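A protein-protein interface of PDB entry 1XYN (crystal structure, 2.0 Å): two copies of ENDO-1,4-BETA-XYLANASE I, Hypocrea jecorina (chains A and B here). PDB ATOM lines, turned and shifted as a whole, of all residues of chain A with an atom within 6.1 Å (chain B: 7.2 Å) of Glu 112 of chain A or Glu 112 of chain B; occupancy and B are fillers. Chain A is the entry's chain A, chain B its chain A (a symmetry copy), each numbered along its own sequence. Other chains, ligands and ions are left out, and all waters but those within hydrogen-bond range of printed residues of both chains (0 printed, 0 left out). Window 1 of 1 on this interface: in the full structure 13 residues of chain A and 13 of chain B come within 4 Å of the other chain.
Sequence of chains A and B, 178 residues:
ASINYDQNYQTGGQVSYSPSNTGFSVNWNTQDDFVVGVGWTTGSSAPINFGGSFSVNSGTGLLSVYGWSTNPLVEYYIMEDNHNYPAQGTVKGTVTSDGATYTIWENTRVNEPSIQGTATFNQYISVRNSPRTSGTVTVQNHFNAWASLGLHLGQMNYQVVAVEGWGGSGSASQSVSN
The side-chain carboxylate of Glu 112 of chain A is in salt-bridge range of the guanidinium group of Arg 109 of chain B (3.0 Å). The guanidinium group (NH1) of Arg 109 of chain A lies within hydrogen-bond range of the backbone carbonyl oxygen (O) of Val 110 of chain B, 2.8 Å away. NH1 of Arg 109 of chain A is in salt-bridge range of OE2 of Glu 112 of chain B (3.0 Å). O of Val 110 of chain A lies within hydrogen-bond range of NH1 of Arg 109 of chain B, 2.8 Å away. OE1 of Glu 112 of chain A sits close to OE1 of Glu 112 of chain B, 2.7 Å away.
The backbone NH of Glu 112 of chain A is in hydrogen-bond range of the backbone carbonyl oxygen of Ala 119 of chain A (2.7 Å). N of Arg 109 of chain A is in hydrogen-bond range of O of Phe 121 of chain A, 2.9 Å away. N of Arg 109 of chain B sits at hydrogen-bond distance from O of Phe 121 of chain B, at 2.9 Å. O of Gly 117 of chain A sits at hydrogen-bond distance from OG of Ser 114 of chain A (2.5 Å). The backbone carbonyl oxygen (O) of Ala 119 of chain A lies within hydrogen-bond range of the backbone NH (N) of Asn 111 of chain A. The backbone carbonyl oxygen (O) of Ala 119 of chain B lies within hydrogen-bond range of the backbone NH (N) of Asn 111 of chain B, at 3.3 Å.
Printed residues of chain B within 4 Å of Arg 109 of chain A: Val 110, Asn 111 and Glu 112. Of the printed residues of chain B, Asn 111 of chain A touches Arg 109. Of chain B, only Arg 109 (3.0 Å) and Glu 112 (2.7 Å) come within 4 Å of Glu 112 of chain A. Of the printed residues of chain B, Thr 118 of chain A touches Asp 32. Phe 121 of chain A touches none of the printed residues of chain B. Of the printed residues of chain A, Val 110 of chain B touches Arg 109 (2.8 Å). Printed residues of chain A within 4 Å of Asn 111 of chain B: Arg 109. Glu 112 of chain B touches just these residues of chain A: Arg 109 and Glu 112. Thr 120 of chain B touches none of the printed residues of chain A. The nearest residue of chain B that does not touch Glu 112 of chain A is Asn 111 of chain B (5.6 Å). The nearest residue of chain A that does not touch Glu 112 of chain B is Asn 111 of chain A (5.6 Å).
Arg 109 of chain A touches Val 110 of chain B, and with the chains exchanged Val 110 of chain A touches Arg 109 of chain B. Arg 109 of chain A touches Asn 111 of chain B, and with the chains exchanged Asn 111 of chain A touches Arg 109 of chain B. Arg 109 of chain A touches Glu 112 of chain B, and with the chains exchanged Glu 112 of chain A touches Arg 109 of chain B. Glu 112 of chain A touches its own counterpart, Glu 112 of chain B. 11 positions are printed for both chains. Of the 9 pairs that touch across the chains among the printed residues, 7 have their exchanged pair printed and touching as well.
Of the 11 printed residues of chain A, 6 touch a printed residue of chain B. Of the 18 printed residues of chain B, 5 touch a printed residue of chain A. Printed residues of chain B that touch a printed residue of chain A: Asp 32, Arg 109, Val 110, Asn 111 and Glu 112. Among the printed residues, 9 pairs touch across the chains.
Among the printed residues, pairs that only touch across the chains: Arg 109 of chain A with Asn 111 of chain B (3.8 Å), Asn 111 of chain A with Arg 109 of chain B (3.8 Å), Gly 117 of chain A with Asp 32 of chain B (3.2 Å) and Thr 118 of chain A with Asp 32 of chain B (3.8 Å).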
ATOM      1  N   ARG A 109      34.023   0.999  -5.139  1.00  0.00           N
ATOM      2  CA  ARG A 109      32.763   0.292  -4.990  1.00  0.00           C
ATOM      3  C   ARG A 109      32.959  -0.730  -3.872  1.00  0.00           C
ATOM      4  O   ARG A 109      33.723  -1.681  -4.020  1.00  0.00           O
ATOM      5  CB  ARG A 109      32.408  -0.398  -6.313  1.00  0.00           C
ATOM      6  CG  ARG A 109      31.863   0.549  -7.381  1.00  0.00           C
ATOM      7  CD  ARG A 109      30.506   1.083  -6.947  1.00  0.00           C
ATOM      8  NE  ARG A 109      29.962   2.106  -7.835  1.00  0.00           N
ATOM      9  CZ  ARG A 109      28.873   2.830  -7.565  1.00  0.00           C
ATOM     10  NH1 ARG A 109      28.204   2.642  -6.431  1.00  0.00           N
ATOM     11  NH2 ARG A 109      28.460   3.760  -8.425  1.00  0.00           N
ATOM     12  N   VAL A 110      32.324  -0.486  -2.729  1.00  0.00           N
ATOM     13  CA  VAL A 110      32.442  -1.387  -1.581  1.00  0.00           C
ATOM     14  C   VAL A 110      31.364  -2.461  -1.586  1.00  0.00           C
ATOM     15  O   VAL A 110      30.179  -2.151  -1.719  1.00  0.00           O
ATOM     16  CB  VAL A 110      32.380  -0.604  -0.245  1.00  0.00           C
ATOM     17  CG1 VAL A 110      32.224  -1.559   0.930  1.00  0.00           C
ATOM     18  CG2 VAL A 110      33.638   0.236  -0.079  1.00  0.00           C
ATOM     19  N   ASN A 111      31.781  -3.718  -1.444  1.00  0.00           N
ATOM     20  CA  ASN A 111      30.860  -4.858  -1.420  1.00  0.00           C
ATOM     21  C   ASN A 111      29.892  -4.810  -2.592  1.00  0.00           C
ATOM     22  O   ASN A 111      28.674  -4.854  -2.409  1.00  0.00           O
ATOM     23  CB  ASN A 111      30.072  -4.886  -0.109  1.00  0.00           C
ATOM     24  CG  ASN A 111      30.966  -5.012   1.106  1.00  0.00           C
ATOM     25  OD1 ASN A 111      31.947  -5.760   1.098  1.00  0.00           O
ATOM     26  ND2 ASN A 111      30.633  -4.276   2.161  1.00  0.00           N
ATOM     27  N   GLU A 112      30.442  -4.657  -3.789  1.00  0.00           N
ATOM     28  CA  GLU A 112      29.648  -4.590  -5.004  1.00  0.00           C
ATOM     29  C   GLU A 112      29.893  -5.825  -5.859  1.00  0.00           C
ATOM     30  O   GLU A 112      30.957  -6.434  -5.804  1.00  0.00           O
ATOM     31  CB  GLU A 112      30.013  -3.336  -5.797  1.00  0.00           C
ATOM     32  CG  GLU A 112      29.792  -2.039  -5.032  1.00  0.00           C
ATOM     33  CD  GLU A 112      28.348  -1.814  -4.631  1.00  0.00           C
ATOM     34  OE1 GLU A 112      27.446  -2.149  -5.436  1.00  0.00           O
ATOM     35  OE2 GLU A 112      28.113  -1.291  -3.519  1.00  0.00           O
ATOM     36  N   PRO A 113      28.898  -6.224  -6.654  1.00  0.00           N
ATOM     37  CA  PRO A 113      29.066  -7.400  -7.506  1.00  0.00           C
ATOM     38  C   PRO A 113      30.177  -7.219  -8.533  1.00  0.00           C
ATOM     39  O   PRO A 113      30.325  -6.146  -9.127  1.00  0.00           O
ATOM     40  CB  PRO A 113      27.691  -7.547  -8.156  1.00  0.00           C
ATOM     41  CG  PRO A 113      27.162  -6.150  -8.168  1.00  0.00           C
ATOM     42  CD  PRO A 113      27.545  -5.661  -6.803  1.00  0.00           C
ATOM     43  N   SER A 114      30.964  -8.273  -8.723  1.00  0.00           N
ATOM     44  CA  SER A 114      32.062  -8.246  -9.678  1.00  0.00           C
ATOM     45  C   SER A 114      32.265  -9.611 -10.302  1.00  0.00           C
ATOM     46  O   SER A 114      31.573 -10.570  -9.959  1.00  0.00           O
ATOM     47  CB  SER A 114      33.362  -7.807  -8.993  1.00  0.00           C
ATOM     48  OG  SER A 114      33.881  -8.833  -8.172  1.00  0.00           O
ATOM     49  N   GLY A 117      32.870 -12.162  -7.775  1.00  0.00           N
ATOM     50  CA  GLY A 117      31.835 -12.278  -6.765  1.00  0.00           C
ATOM     51  C   GLY A 117      31.658 -10.883  -6.193  1.00  0.00           C
ATOM     52  O   GLY A 117      32.173  -9.920  -6.762  1.00  0.00           O
ATOM     53  N   THR A 118      30.914 -10.740  -5.103  1.00  0.00           N
ATOM     54  CA  THR A 118      30.743  -9.416  -4.511  1.00  0.00           C
ATOM     55  C   THR A 118      32.062  -9.046  -3.833  1.00  0.00           C
ATOM     56  O   THR A 118      32.609  -9.816  -3.023  1.00  0.00           O
ATOM     57  CB  THR A 118      29.546  -9.362  -3.540  1.00  0.00           C
ATOM     58  OG1 THR A 118      29.679 -10.375  -2.540  1.00  0.00           O
ATOM     59  CG2 THR A 118      28.250  -9.591  -4.302  1.00  0.00           C
ATOM     60  N   ALA A 119      32.612  -7.905  -4.241  1.00  0.00           N
ATOM     61  CA  ALA A 119      33.892  -7.444  -3.726  1.00  0.00           C
ATOM     62  C   ALA A 119      33.990  -5.928  -3.667  1.00  0.00           C
ATOM     63  O   ALA A 119      33.067  -5.215  -4.047  1.00  0.00           O
ATOM     64  CB  ALA A 119      35.021  -7.994  -4.597  1.00  0.00           C
ATOM     65  N   THR A 120      35.123  -5.454  -3.158  1.00  0.00           N
ATOM     66  CA  THR A 120      35.406  -4.029  -3.051  1.00  0.00           C
ATOM     67  C   THR A 120      36.539  -3.802  -4.033  1.00  0.00           C
ATOM     68  O   THR A 120      37.536  -4.519  -4.008  1.00  0.00           O
ATOM     69  CB  THR A 120      35.836  -3.653  -1.625  1.00  0.00           C
ATOM     70  OG1 THR A 120      34.726  -3.840  -0.738  1.00  0.00           O
ATOM     71  CG2 THR A 120      36.289  -2.198  -1.555  1.00  0.00           C
ATOM     72  N   PHE A 121      36.388  -2.806  -4.895  1.00  0.00           N
ATOM     73  CA  PHE A 121      37.389  -2.541  -5.916  1.00  0.00           C
ATOM     74  C   PHE A 121      37.278  -1.100  -6.390  1.00  0.00           C
ATOM     75  O   PHE A 121      36.301  -0.421  -6.101  1.00  0.00           O
ATOM     76  CB  PHE A 121      37.129  -3.481  -7.094  1.00  0.00           C
ATOM     77  CG  PHE A 121      35.692  -3.473  -7.561  1.00  0.00           C
ATOM     78  CD1 PHE A 121      34.757  -4.326  -6.985  1.00  0.00           C
ATOM     79  CD2 PHE A 121      35.265  -2.574  -8.538  1.00  0.00           C
ATOM     80  CE1 PHE A 121      33.424  -4.281  -7.365  1.00  0.00           C
ATOM     81  CE2 PHE A 121      33.929  -2.521  -8.929  1.00  0.00           C
ATOM     82  CZ  PHE A 121      33.007  -3.373  -8.342  1.00  0.00           C
ATOM     83  N   ASP B  32      28.599 -14.655  -4.306  1.00  0.00           N
ATOM     84  CA  ASP B  32      27.666 -13.554  -4.489  1.00  0.00           C
ATOM     85  C   ASP B  32      26.664 -13.327  -3.361  1.00  0.00           C
ATOM     86  O   ASP B  32      26.151 -14.273  -2.759  1.00  0.00           O
ATOM     87  CB  ASP B  32      26.919 -13.711  -5.815  1.00  0.00           C
ATOM     88  CG  ASP B  32      27.849 -13.869  -6.995  1.00  0.00           C
ATOM     89  OD1 ASP B  32      28.784 -13.060  -7.151  1.00  0.00           O
ATOM     90  OD2 ASP B  32      27.638 -14.808  -7.780  1.00  0.00           O
ATOM     91  N   TRP B  68      13.151  -1.805   5.059  1.00  0.00           N
ATOM     92  CA  TRP B  68      13.198  -0.592   4.256  1.00  0.00           C
ATOM     93  C   TRP B  68      12.204   0.449   4.762  1.00  0.00           C
ATOM     94  O   TRP B  68      11.303   0.153   5.546  1.00  0.00           O
ATOM     95  CB  TRP B  68      12.890  -0.907   2.790  1.00  0.00           C
ATOM     96  CG  TRP B  68      14.005  -1.599   2.097  1.00  0.00           C
ATOM     97  CD1 TRP B  68      14.309  -2.921   2.172  1.00  0.00           C
ATOM     98  CD2 TRP B  68      15.018  -0.996   1.276  1.00  0.00           C
ATOM     99  NE1 TRP B  68      15.455  -3.184   1.459  1.00  0.00           N
ATOM    100  CE2 TRP B  68      15.911  -2.022   0.896  1.00  0.00           C
ATOM    101  CE3 TRP B  68      15.261   0.312   0.825  1.00  0.00           C
ATOM    102  CZ2 TRP B  68      17.031  -1.785   0.090  1.00  0.00           C
ATOM    103  CZ3 TRP B  68      16.373   0.546   0.023  1.00  0.00           C
ATOM    104  CH2 TRP B  68      17.243  -0.498  -0.335  1.00  0.00           C
ATOM    105  N   LEU B  73      14.078   7.253   1.684  1.00  0.00           N
ATOM    106  CA  LEU B  73      14.385   5.857   1.379  1.00  0.00           C
ATOM    107  C   LEU B  73      15.509   5.414   2.319  1.00  0.00           C
ATOM    108  O   LEU B  73      16.611   5.965   2.272  1.00  0.00           O
ATOM    109  CB  LEU B  73      14.816   5.696  -0.087  1.00  0.00           C
ATOM    110  CG  LEU B  73      15.241   4.291  -0.547  1.00  0.00           C
ATOM    111  CD1 LEU B  73      14.100   3.305  -0.369  1.00  0.00           C
ATOM    112  CD2 LEU B  73      15.695   4.323  -1.991  1.00  0.00           C
ATOM    113  N   GLU B  75      17.467   1.862   4.217  1.00  0.00           N
ATOM    114  CA  GLU B  75      17.656   0.427   4.387  1.00  0.00           C
ATOM    115  C   GLU B  75      18.248   0.269   5.784  1.00  0.00           C
ATOM    116  O   GLU B  75      19.289   0.839   6.089  1.00  0.00           O
ATOM    117  CB  GLU B  75      18.631  -0.104   3.344  1.00  0.00           C
ATOM    118  CG  GLU B  75      19.021  -1.563   3.511  1.00  0.00           C
ATOM    119  CD  GLU B  75      19.957  -2.036   2.414  1.00  0.00           C
ATOM    120  OE1 GLU B  75      20.945  -1.330   2.131  1.00  0.00           O
ATOM    121  OE2 GLU B  75      19.699  -3.105   1.822  1.00  0.00           O
ATOM    122  N   THR B 108      26.065   5.162   3.440  1.00  0.00           N
ATOM    123  CA  THR B 108      25.373   5.599   2.249  1.00  0.00           C
ATOM    124  C   THR B 108      25.702   4.639   1.111  1.00  0.00           C
ATOM    125  O   THR B 108      26.828   4.163   0.980  1.00  0.00           O
ATOM    126  CB  THR B 108      25.757   7.047   1.877  1.00  0.00           C
ATOM    127  OG1 THR B 108      25.571   7.892   3.021  1.00  0.00           O
ATOM    128  CG2 THR B 108      24.886   7.565   0.737  1.00  0.00           C
ATOM    129  N   ARG B 109      24.671   4.294   0.353  1.00  0.00           N
ATOM    130  CA  ARG B 109      24.786   3.395  -0.782  1.00  0.00           C
ATOM    131  C   ARG B 109      24.443   4.210  -2.027  1.00  0.00           C
ATOM    132  O   ARG B 109      23.303   4.634  -2.203  1.00  0.00           O
ATOM    133  CB  ARG B 109      23.813   2.223  -0.603  1.00  0.00           C
ATOM    134  CG  ARG B 109      24.284   1.172   0.401  1.00  0.00           C
ATOM    135  CD  ARG B 109      25.515   0.461  -0.142  1.00  0.00           C
ATOM    136  NE  ARG B 109      26.126  -0.467   0.804  1.00  0.00           N
ATOM    137  CZ  ARG B 109      27.301  -1.071   0.608  1.00  0.00           C
ATOM    138  NH1 ARG B 109      27.994  -0.849  -0.505  1.00  0.00           N
ATOM    139  NH2 ARG B 109      27.795  -1.887   1.538  1.00  0.00           N
ATOM    140  N   VAL B 110      25.450   4.490  -2.849  1.00  0.00           N
ATOM    141  CA  VAL B 110      25.248   5.272  -4.069  1.00  0.00           C
ATOM    142  C   VAL B 110      24.930   4.389  -5.267  1.00  0.00           C
ATOM    143  O   VAL B 110      25.649   3.425  -5.535  1.00  0.00           O
ATOM    144  CB  VAL B 110      26.490   6.143  -4.389  1.00  0.00           C
ATOM    145  CG1 VAL B 110      26.385   6.733  -5.788  1.00  0.00           C
ATOM    146  CG2 VAL B 110      26.623   7.253  -3.357  1.00  0.00           C
ATOM    147  N   ASN B 111      23.854   4.721  -5.977  1.00  0.00           N
ATOM    148  CA  ASN B 111      23.427   3.971  -7.163  1.00  0.00           C
ATOM    149  C   ASN B 111      23.365   2.479  -6.878  1.00  0.00           C
ATOM    150  O   ASN B 111      23.977   1.674  -7.583  1.00  0.00           O
ATOM    151  CB  ASN B 111      24.378   4.228  -8.333  1.00  0.00           C
ATOM    152  CG  ASN B 111      24.435   5.688  -8.728  1.00  0.00           C
ATOM    153  OD1 ASN B 111      23.414   6.379  -8.756  1.00  0.00           O
ATOM    154  ND2 ASN B 111      25.636   6.168  -9.037  1.00  0.00           N
ATOM    155  N   GLU B 112      22.671   2.124  -5.805  1.00  0.00           N
ATOM    156  CA  GLU B 112      22.523   0.736  -5.402  1.00  0.00           C
ATOM    157  C   GLU B 112      21.079   0.290  -5.580  1.00  0.00           C
ATOM    158  O   GLU B 112      20.153   1.093  -5.516  1.00  0.00           O
ATOM    159  CB  GLU B 112      22.935   0.571  -3.940  1.00  0.00           C
ATOM    160  CG  GLU B 112      24.372   0.981  -3.657  1.00  0.00           C
ATOM    161  CD  GLU B 112      25.394   0.163  -4.421  1.00  0.00           C
ATOM    162  OE1 GLU B 112      25.182  -1.063  -4.576  1.00  0.00           O
ATOM    163  OE2 GLU B 112      26.415   0.742  -4.857  1.00  0.00           O
ATOM    164  N   PRO B 113      20.866  -1.005  -5.825  1.00  0.00           N
ATOM    165  CA  PRO B 113      19.503  -1.503  -6.003  1.00  0.00           C
ATOM    166  C   PRO B 113      18.651  -1.322  -4.753  1.00  0.00           C
ATOM    167  O   PRO B 113      19.118  -1.533  -3.629  1.00  0.00           O
ATOM    168  CB  PRO B 113      19.724  -2.976  -6.348  1.00  0.00           C
ATOM    169  CG  PRO B 113      21.019  -3.300  -5.676  1.00  0.00           C
ATOM    170  CD  PRO B 113      21.846  -2.091  -5.998  1.00  0.00           C
ATOM    171  N   SER B 114      17.403  -0.914  -4.960  1.00  0.00           N
ATOM    172  CA  SER B 114      16.474  -0.705  -3.859  1.00  0.00           C
ATOM    173  C   SER B 114      15.059  -1.040  -4.280  1.00  0.00           C
ATOM    174  O   SER B 114      14.812  -1.398  -5.433  1.00  0.00           O
ATOM    175  CB  SER B 114      16.526   0.751  -3.380  1.00  0.00           C
ATOM    176  OG  SER B 114      15.892   1.617  -4.299  1.00  0.00           O
ATOM    177  N   ILE B 115      14.132  -0.899  -3.336  1.00  0.00           N
ATOM    178  CA  ILE B 115      12.720  -1.163  -3.570  1.00  0.00           C
ATOM    179  C   ILE B 115      12.126  -0.110  -4.505  1.00  0.00           C
ATOM    180  O   ILE B 115      10.990  -0.244  -4.960  1.00  0.00           O
ATOM    181  CB  ILE B 115      11.921  -1.178  -2.243  1.00  0.00           C
ATOM    182  CG1 ILE B 115      12.132   0.133  -1.480  1.00  0.00           C
ATOM    183  CG2 ILE B 115      12.348  -2.358  -1.387  1.00  0.00           C
ATOM    184  CD1 ILE B 115      11.308   0.250  -0.223  1.00  0.00           C
ATOM    185  N   GLN B 116      12.910   0.932  -4.782  1.00  0.00           N
ATOM    186  CA  GLN B 116      12.505   2.028  -5.663  1.00  0.00           C
ATOM    187  C   GLN B 116      13.320   2.014  -6.956  1.00  0.00           C
ATOM    188  O   GLN B 116      13.262   2.959  -7.756  1.00  0.00           O
ATOM    189  CB  GLN B 116      12.716   3.371  -4.961  1.00  0.00           C
ATOM    190  CG  GLN B 116      12.031   3.485  -3.609  1.00  0.00           C
ATOM    191  CD  GLN B 116      11.850   4.930  -3.162  1.00  0.00           C
ATOM    192  OE1 GLN B 116      12.025   5.870  -3.946  1.00  0.00           O
ATOM    193  NE2 GLN B 116      11.483   5.112  -1.901  1.00  0.00           N
ATOM    194  N   GLY B 117      14.024   0.910  -7.177  1.00  0.00           N
ATOM    195  CA  GLY B 117      14.883   0.778  -8.339  1.00  0.00           C
ATOM    196  C   GLY B 117      16.285   1.101  -7.855  1.00  0.00           C
ATOM    197  O   GLY B 117      16.512   1.178  -6.647  1.00  0.00           O
ATOM    198  N   THR B 118      17.243   1.257  -8.761  1.00  0.00           N
ATOM    199  CA  THR B 118      18.598   1.593  -8.333  1.00  0.00           C
ATOM    200  C   THR B 118      18.585   3.055  -7.886  1.00  0.00           C
ATOM    201  O   THR B 118      18.128   3.950  -8.619  1.00  0.00           O
ATOM    202  CB  THR B 118      19.642   1.325  -9.436  1.00  0.00           C
ATOM    203  OG1 THR B 118      19.279   2.016 -10.634  1.00  0.00           O
ATOM    204  CG2 THR B 118      19.711  -0.166  -9.730  1.00  0.00           C
ATOM    205  N   ALA B 119      19.005   3.274  -6.642  1.00  0.00           N
ATOM    206  CA  ALA B 119      19.003   4.606  -6.056  1.00  0.00           C
ATOM    207  C   ALA B 119      20.131   4.810  -5.058  1.00  0.00           C
ATOM    208  O   ALA B 119      20.920   3.907  -4.794  1.00  0.00           O
ATOM    209  CB  ALA B 119      17.663   4.858  -5.367  1.00  0.00           C
ATOM    210  N   THR B 120      20.205   6.027  -4.528  1.00  0.00           N
ATOM    211  CA  THR B 120      21.202   6.396  -3.532  1.00  0.00           C
ATOM    212  C   THR B 120      20.395   6.627  -2.269  1.00  0.00           C
ATOM    213  O   THR B 120      19.406   7.354  -2.288  1.00  0.00           O
ATOM    214  CB  THR B 120      21.951   7.673  -3.942  1.00  0.00           C
ATOM    215  OG1 THR B 120      22.732   7.401  -5.112  1.00  0.00           O
ATOM    216  CG2 THR B 120      22.875   8.149  -2.825  1.00  0.00           C
ATOM    217  N   PHE B 121      20.817   6.011  -1.173  1.00  0.00           N
ATOM    218  CA  PHE B 121      20.082   6.119   0.077  1.00  0.00           C
ATOM    219  C   PHE B 121      21.003   5.814   1.249  1.00  0.00           C
ATOM    220  O   PHE B 121      22.101   5.304   1.063  1.00  0.00           O
ATOM    221  CB  PHE B 121      18.944   5.099   0.050  1.00  0.00           C
ATOM    222  CG  PHE B 121      19.395   3.707  -0.332  1.00  0.00           C
ATOM    223  CD1 PHE B 121      19.448   3.324  -1.669  1.00  0.00           C
ATOM    224  CD2 PHE B 121      19.818   2.803   0.641  1.00  0.00           C
ATOM    225  CE1 PHE B 121      19.920   2.072  -2.031  1.00  0.00           C
ATOM    226  CE2 PHE B 121      20.292   1.541   0.289  1.00  0.00           C
ATOM    227  CZ  PHE B 121      20.345   1.175  -1.047  1.00  0.00           C
